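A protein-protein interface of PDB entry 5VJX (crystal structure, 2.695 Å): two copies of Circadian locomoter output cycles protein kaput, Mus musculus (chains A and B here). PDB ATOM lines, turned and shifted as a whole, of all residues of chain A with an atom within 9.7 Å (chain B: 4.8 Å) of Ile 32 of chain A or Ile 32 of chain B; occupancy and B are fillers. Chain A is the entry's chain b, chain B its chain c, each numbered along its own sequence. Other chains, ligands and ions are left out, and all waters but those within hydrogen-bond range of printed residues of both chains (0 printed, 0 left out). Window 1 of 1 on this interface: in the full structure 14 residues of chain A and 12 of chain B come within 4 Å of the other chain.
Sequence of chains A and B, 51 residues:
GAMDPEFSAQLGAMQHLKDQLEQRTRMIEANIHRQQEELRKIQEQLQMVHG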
ATOM      1  N   ARG A  24      15.301  15.637  -2.258  1.00  0.00           N
ATOM      2  CA  ARG A  24      15.857  15.332  -3.565  1.00  0.00           C
ATOM      3  C   ARG A  24      17.353  15.161  -3.409  1.00  0.00           C
ATOM      4  O   ARG A  24      17.969  14.293  -4.048  1.00  0.00           O
ATOM      5  CB  ARG A  24      15.577  16.440  -4.565  1.00  0.00           C
ATOM      6  CG  ARG A  24      14.147  16.555  -5.002  1.00  0.00           C
ATOM      7  CD  ARG A  24      14.066  17.672  -5.999  1.00  0.00           C
ATOM      8  NE  ARG A  24      14.916  17.350  -7.140  1.00  0.00           N
ATOM      9  CZ  ARG A  24      15.190  18.184  -8.135  1.00  0.00           C
ATOM     10  NH1 ARG A  24      14.699  19.415  -8.125  1.00  0.00           N
ATOM     11  NH2 ARG A  24      15.974  17.792  -9.128  1.00  0.00           N
ATOM     12  N   THR A  25      17.931  15.972  -2.527  1.00  0.00           N
ATOM     13  CA  THR A  25      19.352  15.846  -2.238  1.00  0.00           C
ATOM     14  C   THR A  25      19.722  14.472  -1.691  1.00  0.00           C
ATOM     15  O   THR A  25      20.682  13.851  -2.151  1.00  0.00           O
ATOM     16  CB  THR A  25      19.800  16.897  -1.215  1.00  0.00           C
ATOM     17  OG1 THR A  25      20.123  18.113  -1.889  1.00  0.00           O
ATOM     18  CG2 THR A  25      21.021  16.430  -0.474  1.00  0.00           C
ATOM     19  N   ARG A  26      18.941  13.968  -0.745  1.00  0.00           N
ATOM     20  CA  ARG A  26      19.291  12.682  -0.157  1.00  0.00           C
ATOM     21  C   ARG A  26      19.017  11.524  -1.107  1.00  0.00           C
ATOM     22  O   ARG A  26      19.698  10.495  -1.061  1.00  0.00           O
ATOM     23  CB  ARG A  26      18.577  12.485   1.173  1.00  0.00           C
ATOM     24  CG  ARG A  26      19.212  13.316   2.269  1.00  0.00           C
ATOM     25  CD  ARG A  26      18.460  13.228   3.568  1.00  0.00           C
ATOM     26  NE  ARG A  26      17.128  13.806   3.507  1.00  0.00           N
ATOM     27  CZ  ARG A  26      16.836  15.023   3.942  1.00  0.00           C
ATOM     28  NH1 ARG A  26      17.789  15.787   4.453  1.00  0.00           N
ATOM     29  NH2 ARG A  26      15.596  15.479   3.862  1.00  0.00           N
ATOM     30  N   MET A  27      18.027  11.700  -1.976  1.00  0.00           N
ATOM     31  CA  MET A  27      17.771  10.707  -3.006  1.00  0.00           C
ATOM     32  C   MET A  27      18.963  10.583  -3.944  1.00  0.00           C
ATOM     33  O   MET A  27      19.468   9.479  -4.192  1.00  0.00           O
ATOM     34  CB  MET A  27      16.507  11.057  -3.784  1.00  0.00           C
ATOM     35  CG  MET A  27      15.254  10.774  -2.998  1.00  0.00           C
ATOM     36  SD  MET A  27      15.268   8.927  -2.386  1.00  0.00           S
ATOM     37  CE  MET A  27      14.217   8.144  -3.835  1.00  0.00           C
ATOM     38  N   ILE A  28      19.428  11.718  -4.457  1.00  0.00           N
ATOM     39  CA  ILE A  28      20.608  11.691  -5.308  1.00  0.00           C
ATOM     40  C   ILE A  28      21.799  11.104  -4.552  1.00  0.00           C
ATOM     41  O   ILE A  28      22.528  10.286  -5.095  1.00  0.00           O
ATOM     42  CB  ILE A  28      20.962  13.082  -5.841  1.00  0.00           C
ATOM     43  CG1 ILE A  28      19.881  13.569  -6.801  1.00  0.00           C
ATOM     44  CG2 ILE A  28      22.287  13.052  -6.574  1.00  0.00           C
ATOM     45  CD1 ILE A  28      20.092  14.987  -7.259  1.00  0.00           C
ATOM     46  N   GLU A  29      21.969  11.477  -3.287  1.00  0.00           N
ATOM     47  CA  GLU A  29      23.093  10.978  -2.491  1.00  0.00           C
ATOM     48  C   GLU A  29      23.088   9.440  -2.419  1.00  0.00           C
ATOM     49  O   GLU A  29      24.131   8.773  -2.601  1.00  0.00           O
ATOM     50  CB  GLU A  29      23.035  11.592  -1.090  1.00  0.00           C
ATOM     51  CG  GLU A  29      23.631  10.742   0.020  1.00  0.00           C
ATOM     52  CD  GLU A  29      23.683  11.467   1.360  1.00  0.00           C
ATOM     53  OE1 GLU A  29      23.645  10.781   2.403  1.00  0.00           O
ATOM     54  OE2 GLU A  29      23.752  12.717   1.377  1.00  0.00           O
ATOM     55  N   ALA A  30      21.901   8.879  -2.198  1.00  0.00           N
ATOM     56  CA  ALA A  30      21.727   7.431  -2.197  1.00  0.00           C
ATOM     57  C   ALA A  30      22.117   6.842  -3.556  1.00  0.00           C
ATOM     58  O   ALA A  30      22.854   5.842  -3.636  1.00  0.00           O
ATOM     59  CB  ALA A  30      20.303   7.075  -1.852  1.00  0.00           C
ATOM     60  N   ASN A  31      21.624   7.477  -4.619  1.00  0.00           N
ATOM     61  CA  ASN A  31      21.936   7.050  -5.980  1.00  0.00           C
ATOM     62  C   ASN A  31      23.441   6.920  -6.189  1.00  0.00           C
ATOM     63  O   ASN A  31      23.949   5.882  -6.638  1.00  0.00           O
ATOM     64  CB  ASN A  31      21.381   8.055  -6.994  1.00  0.00           C
ATOM     65  CG  ASN A  31      19.893   7.911  -7.213  1.00  0.00           C
ATOM     66  OD1 ASN A  31      19.257   7.020  -6.657  1.00  0.00           O
ATOM     67  ND2 ASN A  31      19.324   8.811  -8.009  1.00  0.00           N
ATOM     68  N   ILE A  32      24.151   7.984  -5.834  1.00  0.00           N
ATOM     69  CA  ILE A  32      25.591   8.024  -6.012  1.00  0.00           C
ATOM     70  C   ILE A  32      26.288   6.924  -5.220  1.00  0.00           C
ATOM     71  O   ILE A  32      27.186   6.268  -5.741  1.00  0.00           O
ATOM     72  CB  ILE A  32      26.160   9.395  -5.633  1.00  0.00           C
ATOM     73  CG1 ILE A  32      25.691  10.443  -6.641  1.00  0.00           C
ATOM     74  CG2 ILE A  32      27.672   9.349  -5.592  1.00  0.00           C
ATOM     75  CD1 ILE A  32      26.286  11.805  -6.443  1.00  0.00           C
ATOM     76  N   HIS A  33      25.870   6.675  -3.983  1.00  0.00           N
ATOM     77  CA  HIS A  33      26.527   5.587  -3.250  1.00  0.00           C
ATOM     78  C   HIS A  33      26.318   4.225  -3.899  1.00  0.00           C
ATOM     79  O   HIS A  33      27.249   3.404  -3.950  1.00  0.00           O
ATOM     80  CB  HIS A  33      26.078   5.548  -1.800  1.00  0.00           C
ATOM     81  CG  HIS A  33      26.667   6.643  -0.975  1.00  0.00           C
ATOM     82  ND1 HIS A  33      26.162   7.009   0.251  1.00  0.00           N
ATOM     83  CD2 HIS A  33      27.727   7.450  -1.205  1.00  0.00           C
ATOM     84  CE1 HIS A  33      26.889   7.995   0.744  1.00  0.00           C
ATOM     85  NE2 HIS A  33      27.842   8.284  -0.121  1.00  0.00           N
ATOM     86  N   ARG A  34      25.111   3.980  -4.396  1.00  0.00           N
ATOM     87  CA  ARG A  34      24.862   2.721  -5.083  1.00  0.00           C
ATOM     88  C   ARG A  34      25.823   2.611  -6.265  1.00  0.00           C
ATOM     89  O   ARG A  34      26.454   1.556  -6.476  1.00  0.00           O
ATOM     90  CB  ARG A  34      23.410   2.640  -5.554  1.00  0.00           C
ATOM     91  CG  ARG A  34      23.032   1.341  -6.243  1.00  0.00           C
ATOM     92  CD  ARG A  34      21.583   1.363  -6.737  1.00  0.00           C
ATOM     93  NE  ARG A  34      21.354   2.432  -7.709  1.00  0.00           N
ATOM     94  CZ  ARG A  34      20.673   3.549  -7.462  1.00  0.00           C
ATOM     95  NH1 ARG A  34      20.131   3.753  -6.266  1.00  0.00           N
ATOM     96  NH2 ARG A  34      20.524   4.465  -8.414  1.00  0.00           N
ATOM     97  N   GLN A  35      26.000   3.726  -6.981  1.00  0.00           N
ATOM     98  CA  GLN A  35      26.910   3.740  -8.128  1.00  0.00           C
ATOM     99  C   GLN A  35      28.319   3.406  -7.709  1.00  0.00           C
ATOM    100  O   GLN A  35      29.017   2.680  -8.400  1.00  0.00           O
ATOM    101  CB  GLN A  35      26.956   5.111  -8.809  1.00  0.00           C
ATOM    102  CG  GLN A  35      25.708   5.588  -9.477  1.00  0.00           C
ATOM    103  CD  GLN A  35      25.885   6.982 -10.030  1.00  0.00           C
ATOM    104  OE1 GLN A  35      24.969   7.798  -9.995  1.00  0.00           O
ATOM    105  NE2 GLN A  35      27.074   7.267 -10.536  1.00  0.00           N
ATOM    106  N   GLN A  36      28.736   3.942  -6.572  1.00  0.00           N
ATOM    107  CA  GLN A  36      30.080   3.707  -6.071  1.00  0.00           C
ATOM    108  C   GLN A  36      30.327   2.248  -5.675  1.00  0.00           C
ATOM    109  O   GLN A  36      31.428   1.726  -5.872  1.00  0.00           O
ATOM    110  CB  GLN A  36      30.357   4.655  -4.910  1.00  0.00           C
ATOM    111  CG  GLN A  36      31.806   4.751  -4.531  1.00  0.00           C
ATOM    112  CD  GLN A  36      32.032   5.760  -3.439  1.00  0.00           C
ATOM    113  OE1 GLN A  36      31.086   6.342  -2.912  1.00  0.00           O
ATOM    114  NE2 GLN A  36      33.287   5.958  -3.069  1.00  0.00           N
ATOM    115  N   GLU A  37      29.318   1.573  -5.134  1.00  0.00           N
ATOM    116  CA  GLU A  37      29.521   0.152  -4.852  1.00  0.00           C
ATOM    117  C   GLU A  37      29.598  -0.615  -6.174  1.00  0.00           C
ATOM    118  O   GLU A  37      30.427  -1.523  -6.313  1.00  0.00           O
ATOM    119  CB  GLU A  37      28.444  -0.432  -3.936  1.00  0.00           C
ATOM    120  CG  GLU A  37      28.774  -1.869  -3.428  1.00  0.00           C
ATOM    121  CD  GLU A  37      30.057  -1.983  -2.581  1.00  0.00           C
ATOM    122  OE1 GLU A  37      30.417  -1.013  -1.872  1.00  0.00           O
ATOM    123  OE2 GLU A  37      30.715  -3.052  -2.640  1.00  0.00           O
ATOM    124  N   GLU A  38      28.738  -0.284  -7.139  1.00  0.00           N
ATOM    125  CA  GLU A  38      28.856  -0.949  -8.440  1.00  0.00           C
ATOM    126  C   GLU A  38      30.259  -0.750  -9.008  1.00  0.00           C
ATOM    127  O   GLU A  38      30.843  -1.663  -9.590  1.00  0.00           O
ATOM    128  CB  GLU A  38      27.820  -0.470  -9.450  1.00  0.00           C
ATOM    129  CG  GLU A  38      27.898  -1.311 -10.725  1.00  0.00           C
ATOM    130  CD  GLU A  38      26.735  -1.124 -11.673  1.00  0.00           C
ATOM    131  OE1 GLU A  38      25.800  -0.374 -11.330  1.00  0.00           O
ATOM    132  OE2 GLU A  38      26.766  -1.722 -12.774  1.00  0.00           O
ATOM    133  N   LEU A  39      30.783   0.455  -8.842  1.00  0.00           N
ATOM    134  CA  LEU A  39      32.156   0.756  -9.210  1.00  0.00           C
ATOM    135  C   LEU A  39      33.119  -0.214  -8.581  1.00  0.00           C
ATOM    136  O   LEU A  39      33.977  -0.766  -9.260  1.00  0.00           O
ATOM    137  CB  LEU A  39      32.537   2.160  -8.781  1.00  0.00           C
ATOM    138  CG  LEU A  39      33.834   2.675  -9.393  1.00  0.00           C
ATOM    139  CD1 LEU A  39      33.738   2.740 -10.898  1.00  0.00           C
ATOM    140  CD2 LEU A  39      34.197   4.013  -8.790  1.00  0.00           C
ATOM    141  N   ARG A  40      32.977  -0.428  -7.279  1.00  0.00           N
ATOM    142  CA  ARG A  40      33.891  -1.325  -6.591  1.00  0.00           C
ATOM    143  C   ARG A  40      33.841  -2.725  -7.178  1.00  0.00           C
ATOM    144  O   ARG A  40      34.866  -3.371  -7.385  1.00  0.00           O
ATOM    145  CB  ARG A  40      33.544  -1.397  -5.114  1.00  0.00           C
ATOM    146  CG  ARG A  40      34.510  -2.211  -4.305  1.00  0.00           C
ATOM    147  CD  ARG A  40      34.126  -2.139  -2.847  1.00  0.00           C
ATOM    148  NE  ARG A  40      34.272  -0.780  -2.343  1.00  0.00           N
ATOM    149  CZ  ARG A  40      35.417  -0.246  -1.932  1.00  0.00           C
ATOM    150  NH1 ARG A  40      36.542  -0.953  -1.969  1.00  0.00           N
ATOM    151  NH2 ARG A  40      35.437   1.003  -1.491  1.00  0.00           N
ATOM    152  N   ILE A  42      32.924  -3.582 -10.296  1.00  0.00           N
ATOM    153  CA  ILE A  42      33.555  -3.552 -11.610  1.00  0.00           C
ATOM    154  C   ILE A  42      35.084  -3.555 -11.504  1.00  0.00           C
ATOM    155  O   ILE A  42      35.751  -4.285 -12.214  1.00  0.00           O
ATOM    156  CB  ILE A  42      33.093  -2.340 -12.404  1.00  0.00           C
ATOM    157  CG1 ILE A  42      31.608  -2.452 -12.708  1.00  0.00           C
ATOM    158  CG2 ILE A  42      33.880  -2.202 -13.685  1.00  0.00           C
ATOM    159  CD1 ILE A  42      31.047  -1.238 -13.368  1.00  0.00           C
ATOM    160  N   GLN A  43      35.628  -2.748 -10.602  1.00  0.00           N
ATOM    161  CA  GLN A  43      37.072  -2.668 -10.385  1.00  0.00           C
ATOM    162  C   GLN A  43      37.653  -4.003  -9.889  1.00  0.00           C
ATOM    163  O   GLN A  43      38.775  -4.386 -10.241  1.00  0.00           O
ATOM    164  CB  GLN A  43      37.360  -1.559  -9.382  1.00  0.00           C
ATOM    165  CG  GLN A  43      37.161  -0.166  -9.931  1.00  0.00           C
ATOM    166  CD  GLN A  43      37.347   0.919  -8.883  1.00  0.00           C
ATOM    167  OE1 GLN A  43      36.993   0.744  -7.715  1.00  0.00           O
ATOM    168  NE2 GLN A  43      37.892   2.051  -9.299  1.00  0.00           N
ATOM    169  N   ILE B  28      35.157   7.608 -13.905  1.00  0.00           N
ATOM    170  CA  ILE B  28      33.875   7.424 -13.239  1.00  0.00           C
ATOM    171  C   ILE B  28      34.056   7.739 -11.781  1.00  0.00           C
ATOM    172  O   ILE B  28      33.305   8.525 -11.202  1.00  0.00           O
ATOM    173  CB  ILE B  28      33.328   5.999 -13.377  1.00  0.00           C
ATOM    174  CG1 ILE B  28      32.900   5.730 -14.813  1.00  0.00           C
ATOM    175  CG2 ILE B  28      32.124   5.820 -12.487  1.00  0.00           C
ATOM    176  CD1 ILE B  28      32.518   4.309 -15.055  1.00  0.00           C
ATOM    177  N   GLU B  29      35.132   7.203 -11.222  1.00  0.00           N
ATOM    178  CA  GLU B  29      35.386   7.385  -9.823  1.00  0.00           C
ATOM    179  C   GLU B  29      35.561   8.863  -9.541  1.00  0.00           C
ATOM    180  O   GLU B  29      34.925   9.408  -8.637  1.00  0.00           O
ATOM    181  CB  GLU B  29      36.597   6.580  -9.423  1.00  0.00           C
ATOM    182  CG  GLU B  29      36.926   6.623  -7.970  1.00  0.00           C
ATOM    183  CD  GLU B  29      37.982   5.607  -7.641  1.00  0.00           C
ATOM    184  OE1 GLU B  29      39.177   5.960  -7.668  1.00  0.00           O
ATOM    185  OE2 GLU B  29      37.614   4.440  -7.386  1.00  0.00           O
ATOM    186  N   ALA B  30      36.317   9.531 -10.403  1.00  0.00           N
ATOM    187  CA  ALA B  30      36.528  10.954 -10.240  1.00  0.00           C
ATOM    188  C   ALA B  30      35.193  11.658 -10.242  1.00  0.00           C
ATOM    189  O   ALA B  30      34.898  12.450  -9.350  1.00  0.00           O
ATOM    190  CB  ALA B  30      37.414  11.493 -11.337  1.00  0.00           C
ATOM    191  N   ASN B  31      34.365  11.322 -11.220  1.00  0.00           N
ATOM    192  CA  ASN B  31      33.044  11.910 -11.321  1.00  0.00           C
ATOM    193  C   ASN B  31      32.269  11.745 -10.034  1.00  0.00           C
ATOM    194  O   ASN B  31      31.717  12.712  -9.504  1.00  0.00           O
ATOM    195  CB  ASN B  31      32.291  11.303 -12.487  1.00  0.00           C
ATOM    196  CG  ASN B  31      32.712  11.893 -13.800  1.00  0.00           C
ATOM    197  OD1 ASN B  31      32.296  12.988 -14.164  1.00  0.00           O
ATOM    198  ND2 ASN B  31      33.574  11.184 -14.511  1.00  0.00           N
ATOM    199  N   ILE B  32      32.278  10.524  -9.507  1.00  0.00           N
ATOM    200  CA  ILE B  32      31.534  10.219  -8.294  1.00  0.00           C
ATOM    201  C   ILE B  32      31.984  11.147  -7.176  1.00  0.00           C
ATOM    202  O   ILE B  32      31.166  11.638  -6.411  1.00  0.00           O
ATOM    203  CB  ILE B  32      31.706   8.752  -7.891  1.00  0.00           C
ATOM    204  CG1 ILE B  32      30.995   7.863  -8.908  1.00  0.00           C
ATOM    205  CG2 ILE B  32      31.153   8.509  -6.502  1.00  0.00           C
ATOM    206  CD1 ILE B  32      31.009   6.415  -8.560  1.00  0.00           C
ATOM    207  N   HIS B  33      33.283  11.408  -7.098  1.00  0.00           N
ATOM    208  CA  HIS B  33      33.769  12.336  -6.093  1.00  0.00           C
ATOM    209  C   HIS B  33      33.279  13.758  -6.340  1.00  0.00           C
ATOM    210  O   HIS B  33      32.715  14.383  -5.444  1.00  0.00           O
ATOM    211  CB  HIS B  33      35.292  12.331  -6.059  1.00  0.00           C
ATOM    212  CG  HIS B  33      35.869  11.072  -5.487  1.00  0.00           C
ATOM    213  ND1 HIS B  33      35.683   9.850  -6.067  1.00  0.00           N
ATOM    214  CD2 HIS B  33      36.630  10.873  -4.383  1.00  0.00           C
ATOM    215  CE1 HIS B  33      36.307   8.922  -5.344  1.00  0.00           C
ATOM    216  NE2 HIS B  33      36.884   9.518  -4.327  1.00  0.00           N
ATOM    217  N   ARG B  34      33.400  14.230  -7.575  1.00  0.00           N
ATOM    218  CA  ARG B  34      33.000  15.595  -7.877  1.00  0.00           C
ATOM    219  C   ARG B  34      31.534  15.798  -7.595  1.00  0.00           C
ATOM    220  O   ARG B  34      31.144  16.754  -6.916  1.00  0.00           O
ATOM    221  CB  ARG B  34      33.261  15.932  -9.340  1.00  0.00           C
ATOM    222  CG  ARG B  34      32.896  17.358  -9.702  1.00  0.00           C
ATOM    223  CD  ARG B  34      33.056  17.623 -11.197  1.00  0.00           C
ATOM    224  NE  ARG B  34      32.164  16.784 -11.995  1.00  0.00           N
ATOM    225  CZ  ARG B  34      32.567  15.735 -12.703  1.00  0.00           C
ATOM    226  NH1 ARG B  34      33.848  15.387 -12.701  1.00  0.00           N
ATOM    227  NH2 ARG B  34      31.690  15.024 -13.400  1.00  0.00           N
ATOM    228  N   GLN B  35      30.739  14.837  -8.048  1.00  0.00           N
ATOM    229  CA  GLN B  35      29.304  14.885  -7.886  1.00  0.00           C
ATOM    230  C   GLN B  35      28.970  14.914  -6.401  1.00  0.00           C
ATOM    231  O   GLN B  35      28.007  15.555  -5.998  1.00  0.00           O
ATOM    232  CB  GLN B  35      28.631  13.712  -8.615  1.00  0.00           C
ATOM    233  CG  GLN B  35      28.778  13.778 -10.142  1.00  0.00           C
ATOM    234  CD  GLN B  35      28.177  12.589 -10.868  1.00  0.00           C
ATOM    235  OE1 GLN B  35      26.973  12.376 -10.835  1.00  0.00           O
ATOM    236  NE2 GLN B  35      29.018  11.821 -11.542  1.00  0.00           N
ATOM    237  N   GLN B  36      29.748  14.223  -5.580  1.00  0.00           N
ATOM    238  CA  GLN B  36      29.473  14.267  -4.153  1.00  0.00           C
ATOM    239  C   GLN B  36      29.697  15.657  -3.560  1.00  0.00           C
ATOM    240  O   GLN B  36      28.867  16.147  -2.800  1.00  0.00           O
ATOM    241  CB  GLN B  36      30.339  13.247  -3.426  1.00  0.00           C
ATOM    242  CG  GLN B  36      29.888  11.815  -3.590  1.00  0.00           C
ATOM    243  CD  GLN B  36      30.793  10.860  -2.857  1.00  0.00           C
ATOM    244  OE1 GLN B  36      31.917  11.214  -2.509  1.00  0.00           O
ATOM    245  NE2 GLN B  36      30.321   9.643  -2.622  1.00  0.00           N
ATOM    246  N   LEU B  39      26.967  17.904  -4.328  1.00  0.00           N
ATOM    247  CA  LEU B  39      25.901  17.551  -3.396  1.00  0.00           C
ATOM    248  C   LEU B  39      26.096  18.250  -2.080  1.00  0.00           C
ATOM    249  O   LEU B  39      25.190  18.903  -1.572  1.00  0.00           O
ATOM    250  CB  LEU B  39      25.843  16.044  -3.145  1.00  0.00           C
ATOM    251  CG  LEU B  39      25.098  15.158  -4.129  1.00  0.00           C
ATOM    252  CD1 LEU B  39      25.120  13.727  -3.642  1.00  0.00           C
ATOM    253  CD2 LEU B  39      23.684  15.642  -4.244  1.00  0.00           C
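Of the printed residues of chain A, Ile 32 of chain B touches Ile 32 (3.7 Å), Gln 36 (3.8 Å) and Leu 39 (3.998 Å). Ala 30 of chain B touches none of the printed residues of chain A. Asn 31 of chain B touches none of the printed residues of chain A. Of the printed residues of chain A, Gln 35 of chain B touches Ile 32 (3.7 Å). Printed residues of chain B within 4 Å of His 33 of chain A: Gln 36 (3.7 Å). Of the printed residues of chain A, Glu 29 of chain B touches Leu 39 and Gln 43. Printed residues of chain B within 4 Å of Glu 29 of chain A: Leu 39. Of the printed residues of chain B, Leu 39 of chain A touches Ile 28 (3.8 Å), Glu 29 (3.6 Å) and Ile 32 (3.998 Å). Glu 37 of chain A touches none of the printed residues of chain B.
The backbone carbonyl oxygen of Glu 29 of chain B lies within hydrogen-bond range of a ring nitrogen (ND1) of His 33 of chain B, 2.7 Å away. The backbone carbonyl oxygen (O) of Asn 31 of chain B lies close to the side-chain amide nitrogen (NE2) of Gln 35 of chain B.
Of the 10 printed residues of chain B, 6 touch a printed residue of chain A. Hydrophobic or aromatic side chains of chain A that line the printed part of chain B: Ile 28, Ile 32, His 33 and Leu 39.
Glu 29 of chain A touches Leu 39 of chain B, and with the chains exchanged Leu 39 of chain A touches Glu 29 of chain B. Ile 32 of chain B touches its own counterpart, Ile 32 of chain A. His 33 of chain A touches Gln 36 of chain B, but with the chains exchanged Gln 36 of chain A does not touch His 33 of chain B (4.8 Å). Gln 36 of chain B touches its own counterpart, Gln 36 of chain A. 10 positions are printed for both chains. Of the 13 pairs that touch across the chains among the printed residues, 10 have their exchanged pair printed and touching as well.
Ile 28 of chain A touches Leu 39 of chain B (CG2 to CD2, 3.8 Å). CD1 of Leu 39 of chain B touches CA of Glu 29 of chain A, at 3.6 Å. Ile 32 of chain A touches Ile 32 of chain B (CG2 to CG2, 3.7 Å). Ile 32 of chain A touches Gln 35 of chain B. CG2 of Ile 32 of chain A touches CG of Gln 36 of chain B (3.9 Å). Ile 32 of chain A touches Leu 39 of chain B (CD1 to CD1, 3.6 Å). NE2 of Gln 36 of chain B touches CD2 of His 33 of chain A (3.7 Å). Ile 28 of chain B touches Leu 39 of chain A (CG2 to CD1, 3.8 Å). CB of Glu 29 of chain B touches CD2 of Leu 39 of chain A, 3.6 Å away. Leu 39 of chain A touches Ile 32 of chain B (CD2 to CD1, 3.998 Å).
The side-chain amide oxygen of Gln 36 of chain A sits at hydrogen-bond distance from the side-chain amide nitrogen of Gln 36 of chain B. The side-chain carboxylate (OE2) of Glu 29 of chain B lies within hydrogen-bond range of the side-chain amide nitrogen (NE2) of Gln 43 of chain A (3.1 Å).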
